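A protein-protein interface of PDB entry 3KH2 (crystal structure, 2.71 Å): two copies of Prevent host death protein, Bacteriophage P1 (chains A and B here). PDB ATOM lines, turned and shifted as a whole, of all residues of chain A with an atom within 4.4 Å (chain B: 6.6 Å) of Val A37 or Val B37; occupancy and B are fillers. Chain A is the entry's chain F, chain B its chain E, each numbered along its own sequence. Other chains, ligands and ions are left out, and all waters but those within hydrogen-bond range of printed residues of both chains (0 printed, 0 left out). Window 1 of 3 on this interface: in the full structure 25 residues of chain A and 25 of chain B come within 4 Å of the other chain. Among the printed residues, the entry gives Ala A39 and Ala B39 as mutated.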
ATOM      1  N   VAL A  26      -5.541  -3.772  -9.419  1.00  0.00           N
ATOM      2  CA  VAL A  26      -6.951  -3.838  -9.786  1.00  0.00           C
ATOM      3  C   VAL A  26      -7.187  -4.642 -11.063  1.00  0.00           C
ATOM      4  O   VAL A  26      -6.536  -4.402 -12.075  1.00  0.00           O
ATOM      5  CB  VAL A  26      -7.520  -2.420  -9.982  1.00  0.00           C
ATOM      6  CG1 VAL A  26      -9.003  -2.472 -10.283  1.00  0.00           C
ATOM      7  CG2 VAL A  26      -7.260  -1.568  -8.746  1.00  0.00           C
ATOM      8  N   ALA A  36      -8.100  -8.039 -17.931  1.00  0.00           N
ATOM      9  CA  ALA A  36      -6.796  -7.400 -17.823  1.00  0.00           C
ATOM     10  C   ALA A  36      -6.556  -6.984 -16.380  1.00  0.00           C
ATOM     11  O   ALA A  36      -7.459  -7.055 -15.552  1.00  0.00           O
ATOM     12  CB  ALA A  36      -6.733  -6.189 -18.734  1.00  0.00           C
ATOM     13  N   VAL A  37      -5.333  -6.554 -16.090  1.00  0.00           N
ATOM     14  CA  VAL A  37      -4.957  -6.097 -14.756  1.00  0.00           C
ATOM     15  C   VAL A  37      -4.178  -4.793 -14.855  1.00  0.00           C
ATOM     16  O   VAL A  37      -3.363  -4.626 -15.754  1.00  0.00           O
ATOM     17  CB  VAL A  37      -4.094  -7.145 -14.021  1.00  0.00           C
ATOM     18  CG1 VAL A  37      -3.544  -6.576 -12.720  1.00  0.00           C
ATOM     19  CG2 VAL A  37      -4.895  -8.410 -13.752  1.00  0.00           C
ATOM     20  N   ILE A  38      -4.446  -3.873 -13.935  1.00  0.00           N
ATOM     21  CA  ILE A  38      -3.674  -2.642 -13.812  1.00  0.00           C
ATOM     22  C   ILE A  38      -2.828  -2.705 -12.550  1.00  0.00           C
ATOM     23  O   ILE A  38      -3.327  -3.057 -11.483  1.00  0.00           O
ATOM     24  CB  ILE A  38      -4.564  -1.391 -13.707  1.00  0.00           C
ATOM     25  CG1 ILE A  38      -5.687  -1.422 -14.740  1.00  0.00           C
ATOM     26  CG2 ILE A  38      -3.728  -0.124 -13.886  1.00  0.00           C
ATOM     27  CD1 ILE A  38      -6.493  -0.137 -14.782  1.00  0.00           C
ATOM     28  N   ALA A  39      -1.552  -2.352 -12.676  1.00  0.00           N
ATOM     29  CA  ALA A  39      -0.650  -2.251 -11.530  1.00  0.00           C
ATOM     30  C   ALA A  39       0.317  -1.093 -11.733  1.00  0.00           C
ATOM     31  O   ALA A  39       0.441  -0.568 -12.838  1.00  0.00           O
ATOM     32  CB  ALA A  39       0.111  -3.544 -11.347  1.00  0.00           C
ATOM     33  N   LYS A  41       3.882   0.764 -12.261  1.00  0.00           N
ATOM     34  CA  LYS A  41       4.996   0.375 -13.125  1.00  0.00           C
ATOM     35  C   LYS A  41       6.105  -0.310 -12.334  1.00  0.00           C
ATOM     36  O   LYS A  41       6.661  -1.307 -12.783  1.00  0.00           O
ATOM     37  CB  LYS A  41       5.566   1.581 -13.876  1.00  0.00           C
ATOM     38  CG  LYS A  41       6.515   1.194 -15.014  1.00  0.00           C
ATOM     39  CD  LYS A  41       7.098   2.413 -15.704  1.00  0.00           C
ATOM     40  CE  LYS A  41       8.023   2.022 -16.850  1.00  0.00           C
ATOM     41  NZ  LYS A  41       8.575   3.224 -17.545  1.00  0.00           N
ATOM     42  N   PHE A  44       5.013  -3.944 -11.386  1.00  0.00           N
ATOM     43  CA  PHE A  44       4.939  -4.691 -12.633  1.00  0.00           C
ATOM     44  C   PHE A  44       6.337  -5.053 -13.117  1.00  0.00           C
ATOM     45  O   PHE A  44       6.647  -6.227 -13.289  1.00  0.00           O
ATOM     46  CB  PHE A  44       4.218  -3.900 -13.716  1.00  0.00           C
ATOM     47  CG  PHE A  44       4.111  -4.636 -15.015  1.00  0.00           C
ATOM     48  CD1 PHE A  44       3.093  -5.554 -15.216  1.00  0.00           C
ATOM     49  CD2 PHE A  44       5.029  -4.427 -16.029  1.00  0.00           C
ATOM     50  CE1 PHE A  44       2.986  -6.247 -16.406  1.00  0.00           C
ATOM     51  CE2 PHE A  44       4.929  -5.116 -17.222  1.00  0.00           C
ATOM     52  CZ  PHE A  44       3.905  -6.030 -17.409  1.00  0.00           C
ATOM     53  N   VAL B  20      -3.957  -5.188 -25.342  1.00  0.00           N
ATOM     54  CA  VAL B  20      -3.493  -5.925 -24.164  1.00  0.00           C
ATOM     55  C   VAL B  20      -3.622  -7.436 -24.342  1.00  0.00           C
ATOM     56  O   VAL B  20      -2.689  -8.181 -24.052  1.00  0.00           O
ATOM     57  CB  VAL B  20      -4.271  -5.501 -22.893  1.00  0.00           C
ATOM     58  CG1 VAL B  20      -4.181  -6.568 -21.812  1.00  0.00           C
ATOM     59  CG2 VAL B  20      -3.754  -4.171 -22.376  1.00  0.00           C
ATOM     60  N   GLU B  25       1.835  -4.660 -23.588  1.00  0.00           N
ATOM     61  CA  GLU B  25       1.879  -4.235 -22.198  1.00  0.00           C
ATOM     62  C   GLU B  25       1.910  -2.713 -22.188  1.00  0.00           C
ATOM     63  O   GLU B  25       2.955  -2.106 -22.423  1.00  0.00           O
ATOM     64  CB  GLU B  25       3.118  -4.801 -21.505  1.00  0.00           C
ATOM     65  CG  GLU B  25       3.193  -6.327 -21.509  1.00  0.00           C
ATOM     66  CD  GLU B  25       4.482  -6.869 -20.906  1.00  0.00           C
ATOM     67  OE1 GLU B  25       5.469  -6.112 -20.790  1.00  0.00           O
ATOM     68  OE2 GLU B  25       4.511  -8.063 -20.547  1.00  0.00           O
ATOM     69  N   VAL B  26       0.758  -2.105 -21.925  1.00  0.00           N
ATOM     70  CA  VAL B  26       0.590  -0.658 -22.056  1.00  0.00           C
ATOM     71  C   VAL B  26       0.831   0.095 -20.749  1.00  0.00           C
ATOM     72  O   VAL B  26       0.242  -0.226 -19.723  1.00  0.00           O
ATOM     73  CB  VAL B  26      -0.822  -0.323 -22.561  1.00  0.00           C
ATOM     74  CG1 VAL B  26      -1.039   1.180 -22.594  1.00  0.00           C
ATOM     75  CG2 VAL B  26      -1.035  -0.926 -23.934  1.00  0.00           C
ATOM     76  N   GLU B  27       1.703   1.101 -20.811  1.00  0.00           N
ATOM     77  CA  GLU B  27       1.929   2.032 -19.706  1.00  0.00           C
ATOM     78  C   GLU B  27       0.865   3.124 -19.737  1.00  0.00           C
ATOM     79  O   GLU B  27       0.384   3.495 -20.808  1.00  0.00           O
ATOM     80  CB  GLU B  27       3.321   2.671 -19.816  1.00  0.00           C
ATOM     81  CG  GLU B  27       3.738   3.505 -18.601  1.00  0.00           C
ATOM     82  CD  GLU B  27       5.202   3.940 -18.637  1.00  0.00           C
ATOM     83  OE1 GLU B  27       6.035   3.226 -19.229  1.00  0.00           O
ATOM     84  OE2 GLU B  27       5.523   4.996 -18.055  1.00  0.00           O
ATOM     85  N   ILE B  28       0.500   3.630 -18.563  1.00  0.00           N
ATOM     86  CA  ILE B  28      -0.439   4.747 -18.458  1.00  0.00           C
ATOM     87  C   ILE B  28       0.168   5.841 -17.586  1.00  0.00           C
ATOM     88  O   ILE B  28       0.296   5.688 -16.370  1.00  0.00           O
ATOM     89  CB  ILE B  28      -1.802   4.315 -17.891  1.00  0.00           C
ATOM     90  CG1 ILE B  28      -2.408   3.211 -18.759  1.00  0.00           C
ATOM     91  CG2 ILE B  28      -2.753   5.505 -17.839  1.00  0.00           C
ATOM     92  CD1 ILE B  28      -3.834   2.871 -18.407  1.00  0.00           C
ATOM     93  N   PRO B  35       3.599   6.476 -13.130  1.00  0.00           N
ATOM     94  CA  PRO B  35       2.719   5.737 -14.037  1.00  0.00           C
ATOM     95  C   PRO B  35       2.306   4.330 -13.583  1.00  0.00           C
ATOM     96  O   PRO B  35       2.854   3.781 -12.625  1.00  0.00           O
ATOM     97  CB  PRO B  35       3.557   5.638 -15.313  1.00  0.00           C
ATOM     98  CG  PRO B  35       4.950   5.576 -14.825  1.00  0.00           C
ATOM     99  CD  PRO B  35       5.001   6.433 -13.589  1.00  0.00           C
ATOM    100  N   ALA B  36       1.335   3.774 -14.302  1.00  0.00           N
ATOM    101  CA  ALA B  36       0.852   2.411 -14.100  1.00  0.00           C
ATOM    102  C   ALA B  36       1.035   1.611 -15.385  1.00  0.00           C
ATOM    103  O   ALA B  36       1.476   2.148 -16.400  1.00  0.00           O
ATOM    104  CB  ALA B  36      -0.612   2.434 -13.707  1.00  0.00           C
ATOM    105  N   VAL B  37       0.697   0.326 -15.336  1.00  0.00           N
ATOM    106  CA  VAL B  37       0.790  -0.543 -16.507  1.00  0.00           C
ATOM    107  C   VAL B  37      -0.406  -1.487 -16.589  1.00  0.00           C
ATOM    108  O   VAL B  37      -0.708  -2.186 -15.625  1.00  0.00           O
ATOM    109  CB  VAL B  37       2.077  -1.393 -16.476  1.00  0.00           C
ATOM    110  CG1 VAL B  37       2.082  -2.399 -17.611  1.00  0.00           C
ATOM    111  CG2 VAL B  37       3.307  -0.506 -16.548  1.00  0.00           C
ATOM    112  N   ILE B  38      -1.078  -1.500 -17.738  1.00  0.00           N
ATOM    113  CA  ILE B  38      -2.126  -2.479 -18.016  1.00  0.00           C
ATOM    114  C   ILE B  38      -1.525  -3.653 -18.774  1.00  0.00           C
ATOM    115  O   ILE B  38      -0.726  -3.462 -19.686  1.00  0.00           O
ATOM    116  CB  ILE B  38      -3.270  -1.888 -18.857  1.00  0.00           C
ATOM    117  CG1 ILE B  38      -3.819  -0.627 -18.197  1.00  0.00           C
ATOM    118  CG2 ILE B  38      -4.390  -2.905 -19.027  1.00  0.00           C
ATOM    119  CD1 ILE B  38      -5.158  -0.191 -18.752  1.00  0.00           C
ATOM    120  N   ALA B  39      -1.912  -4.862 -18.384  1.00  0.00           N
ATOM    121  CA  ALA B  39      -1.461  -6.084 -19.046  1.00  0.00           C
ATOM    122  C   ALA B  39      -2.486  -7.185 -18.850  1.00  0.00           C
ATOM    123  O   ALA B  39      -3.336  -7.094 -17.970  1.00  0.00           O
ATOM    124  CB  ALA B  39      -0.121  -6.516 -18.490  1.00  0.00           C
ATOM    125  N   SER B  40      -2.400  -8.229 -19.667  1.00  0.00           N
ATOM    126  CA  SER B  40      -3.324  -9.355 -19.555  1.00  0.00           C
ATOM    127  C   SER B  40      -3.158 -10.039 -18.201  1.00  0.00           C
ATOM    128  O   SER B  40      -2.049 -10.133 -17.679  1.00  0.00           O
ATOM    129  CB  SER B  40      -3.103 -10.368 -20.686  1.00  0.00           C
ATOM    130  OG  SER B  40      -2.036 -11.256 -20.392  1.00  0.00           O
ATOM    131  N   LYS B  41      -4.265 -10.513 -17.639  1.00  0.00           N
ATOM    132  CA  LYS B  41      -4.234 -11.208 -16.354  1.00  0.00           C
ATOM    133  C   LYS B  41      -3.348 -12.450 -16.427  1.00  0.00           C
ATOM    134  O   LYS B  41      -2.683 -12.800 -15.454  1.00  0.00           O
ATOM    135  CB  LYS B  41      -5.645 -11.601 -15.907  1.00  0.00           C
ATOM    136  CG  LYS B  41      -5.729 -12.000 -14.436  1.00  0.00           C
ATOM    137  CD  LYS B  41      -7.025 -12.718 -14.101  1.00  0.00           C
ATOM    138  CE  LYS B  41      -6.995 -13.251 -12.679  1.00  0.00           C
ATOM    139  NZ  LYS B  41      -8.310 -13.796 -12.252  1.00  0.00           N
ATOM    140  N   ALA B  42      -3.344 -13.105 -17.584  1.00  0.00           N
ATOM    141  CA  ALA B  42      -2.547 -14.307 -17.794  1.00  0.00           C
ATOM    142  C   ALA B  42      -1.056 -14.039 -17.610  1.00  0.00           C
ATOM    143  O   ALA B  42      -0.378 -14.782 -16.896  1.00  0.00           O
ATOM    144  CB  ALA B  42      -2.807 -14.880 -19.176  1.00  0.00           C
ATOM    145  N   PHE B  44       0.363 -11.123 -16.356  1.00  0.00           N
ATOM    146  CA  PHE B  44       0.575 -10.518 -15.036  1.00  0.00           C
ATOM    147  C   PHE B  44       0.711 -11.589 -13.951  1.00  0.00           C
ATOM    148  O   PHE B  44       1.656 -11.565 -13.173  1.00  0.00           O
ATOM    149  CB  PHE B  44      -0.556  -9.546 -14.673  1.00  0.00           C
ATOM    150  CG  PHE B  44      -0.392  -8.903 -13.318  1.00  0.00           C
ATOM    151  CD1 PHE B  44       0.268  -7.694 -13.185  1.00  0.00           C
ATOM    152  CD2 PHE B  44      -0.890  -9.518 -12.169  1.00  0.00           C
ATOM    153  CE1 PHE B  44       0.425  -7.105 -11.934  1.00  0.00           C
ATOM    154  CE2 PHE B  44      -0.733  -8.936 -10.916  1.00  0.00           C
ATOM    155  CZ  PHE B  44      -0.075  -7.729 -10.800  1.00  0.00           C
ATOM    156  N   GLU B  45      -0.226 -12.527 -13.910  1.00  0.00           N
ATOM    157  CA  GLU B  45      -0.213 -13.584 -12.897  1.00  0.00           C
ATOM    158  C   GLU B  45       1.031 -14.463 -12.992  1.00  0.00           C
ATOM    159  O   GLU B  45       1.551 -14.914 -11.977  1.00  0.00           O
ATOM    160  CB  GLU B  45      -1.467 -14.456 -13.002  1.00  0.00           C
ATOM    161  CG  GLU B  45      -2.761 -13.770 -12.557  1.00  0.00           C
ATOM    162  CD  GLU B  45      -3.059 -13.942 -11.071  1.00  0.00           C
ATOM    163  OE1 GLU B  45      -2.145 -13.732 -10.239  1.00  0.00           O
ATOM    164  OE2 GLU B  45      -4.218 -14.280 -10.735  1.00  0.00           O
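The backbone carbonyl oxygen (O) of Ala B39 sits at hydrogen-bond distance from the backbone NH (N) of Val A37 (2.8 Å).
The backbone NH (N) of Lys A41 is in hydrogen-bond range of the backbone carbonyl oxygen (O) of Pro B35 (3.2 Å).
The backbone carbonyl oxygen of Ala A39 sits at hydrogen-bond distance from the backbone NH of Val B37 (2.7 Å).
The side-chain amino group (NZ) of Lys A41 lies within salt-bridge range of the side-chain carboxylate (OE1) of Glu B27, 3.0 Å away.
The backbone carbonyl oxygen of Val A26 sits at hydrogen-bond distance from the backbone NH of Ile A38 (2.8 Å).
The backbone carbonyl oxygen (O) of Ala B36 is in hydrogen-bond range of the backbone NH (N) of Ile B28.
The backbone carbonyl oxygen of Val B26 sits at hydrogen-bond distance from the backbone NH of Ile B38.
Among the printed residues, pairs that only touch across the chains: Ala A39 with Ala B36 (3.3 Å), Val A37 with Ile B38 (3.4 Å), Ala A36 with Ala B39 (3.5 Å), Ile A38 with Val B37 (3.5 Å), Val A37 with Val B37 (3.6 Å), Ala A39 with Phe B44 (3.6 Å), Phe A44 with Glu B25 (3.6 Å), Val A37 with Lys B41 (3.7 Å), Phe A44 with Ala B39 (3.8 Å), Lys A41 with Ala B36 (3.9 Å), Phe A44 with Val B37 (3.9 Å), Lys A41 with Val B37 (3.9 Å) and Val A37 with Phe B44 (3.96 Å).
Of the printed residues of chain B, Ala A39 touches Ala B36 (3.3 Å), Val B37 (2.7 Å) and Phe B44 (3.6 Å).
Ile B28 touches none of the printed residues of chain A.
Val B37 touches just these residues of chain A: Val A37, Ile A38, Ala A39, Lys A41 and Phe A44.
Printed residues of chain A within 4 Å of Lys B41: Val A37 (3.7 Å).
Ala B42 touches none of the printed residues of chain A.
Of the printed residues of chain A, Phe B44 touches Val A37 and Ala A39.
The nearest printed residue of chain A that does not touch Val B37 is Val A26 (7.2 Å).
Of the 15 printed residues of chain B, 9 touch a printed residue of chain A.
Hydrophobic or aromatic side chains of chain B within 4 Å of the printed part of chain A: Pro B35, Ala B36, Val B37, Ile B38, Ala B39 and Phe B44.
Val A37 touches Ala B39, and with the chains exchanged Ala A39 touches Val B37.
Val A37 touches Lys B41, and with the chains exchanged Lys A41 touches Val B37.
Val A37 touches Phe B44, and with the chains exchanged Phe A44 touches Val B37.
Ala A39 touches Phe B44, and with the chains exchanged Phe A44 touches Ala B39.
Positions printed for both chains: 26, 36, 37, 38, 39, 41 and 44.
Of the 17 pairs that touch across the chains among the printed residues, 13 have their exchanged pair printed and touching as well.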
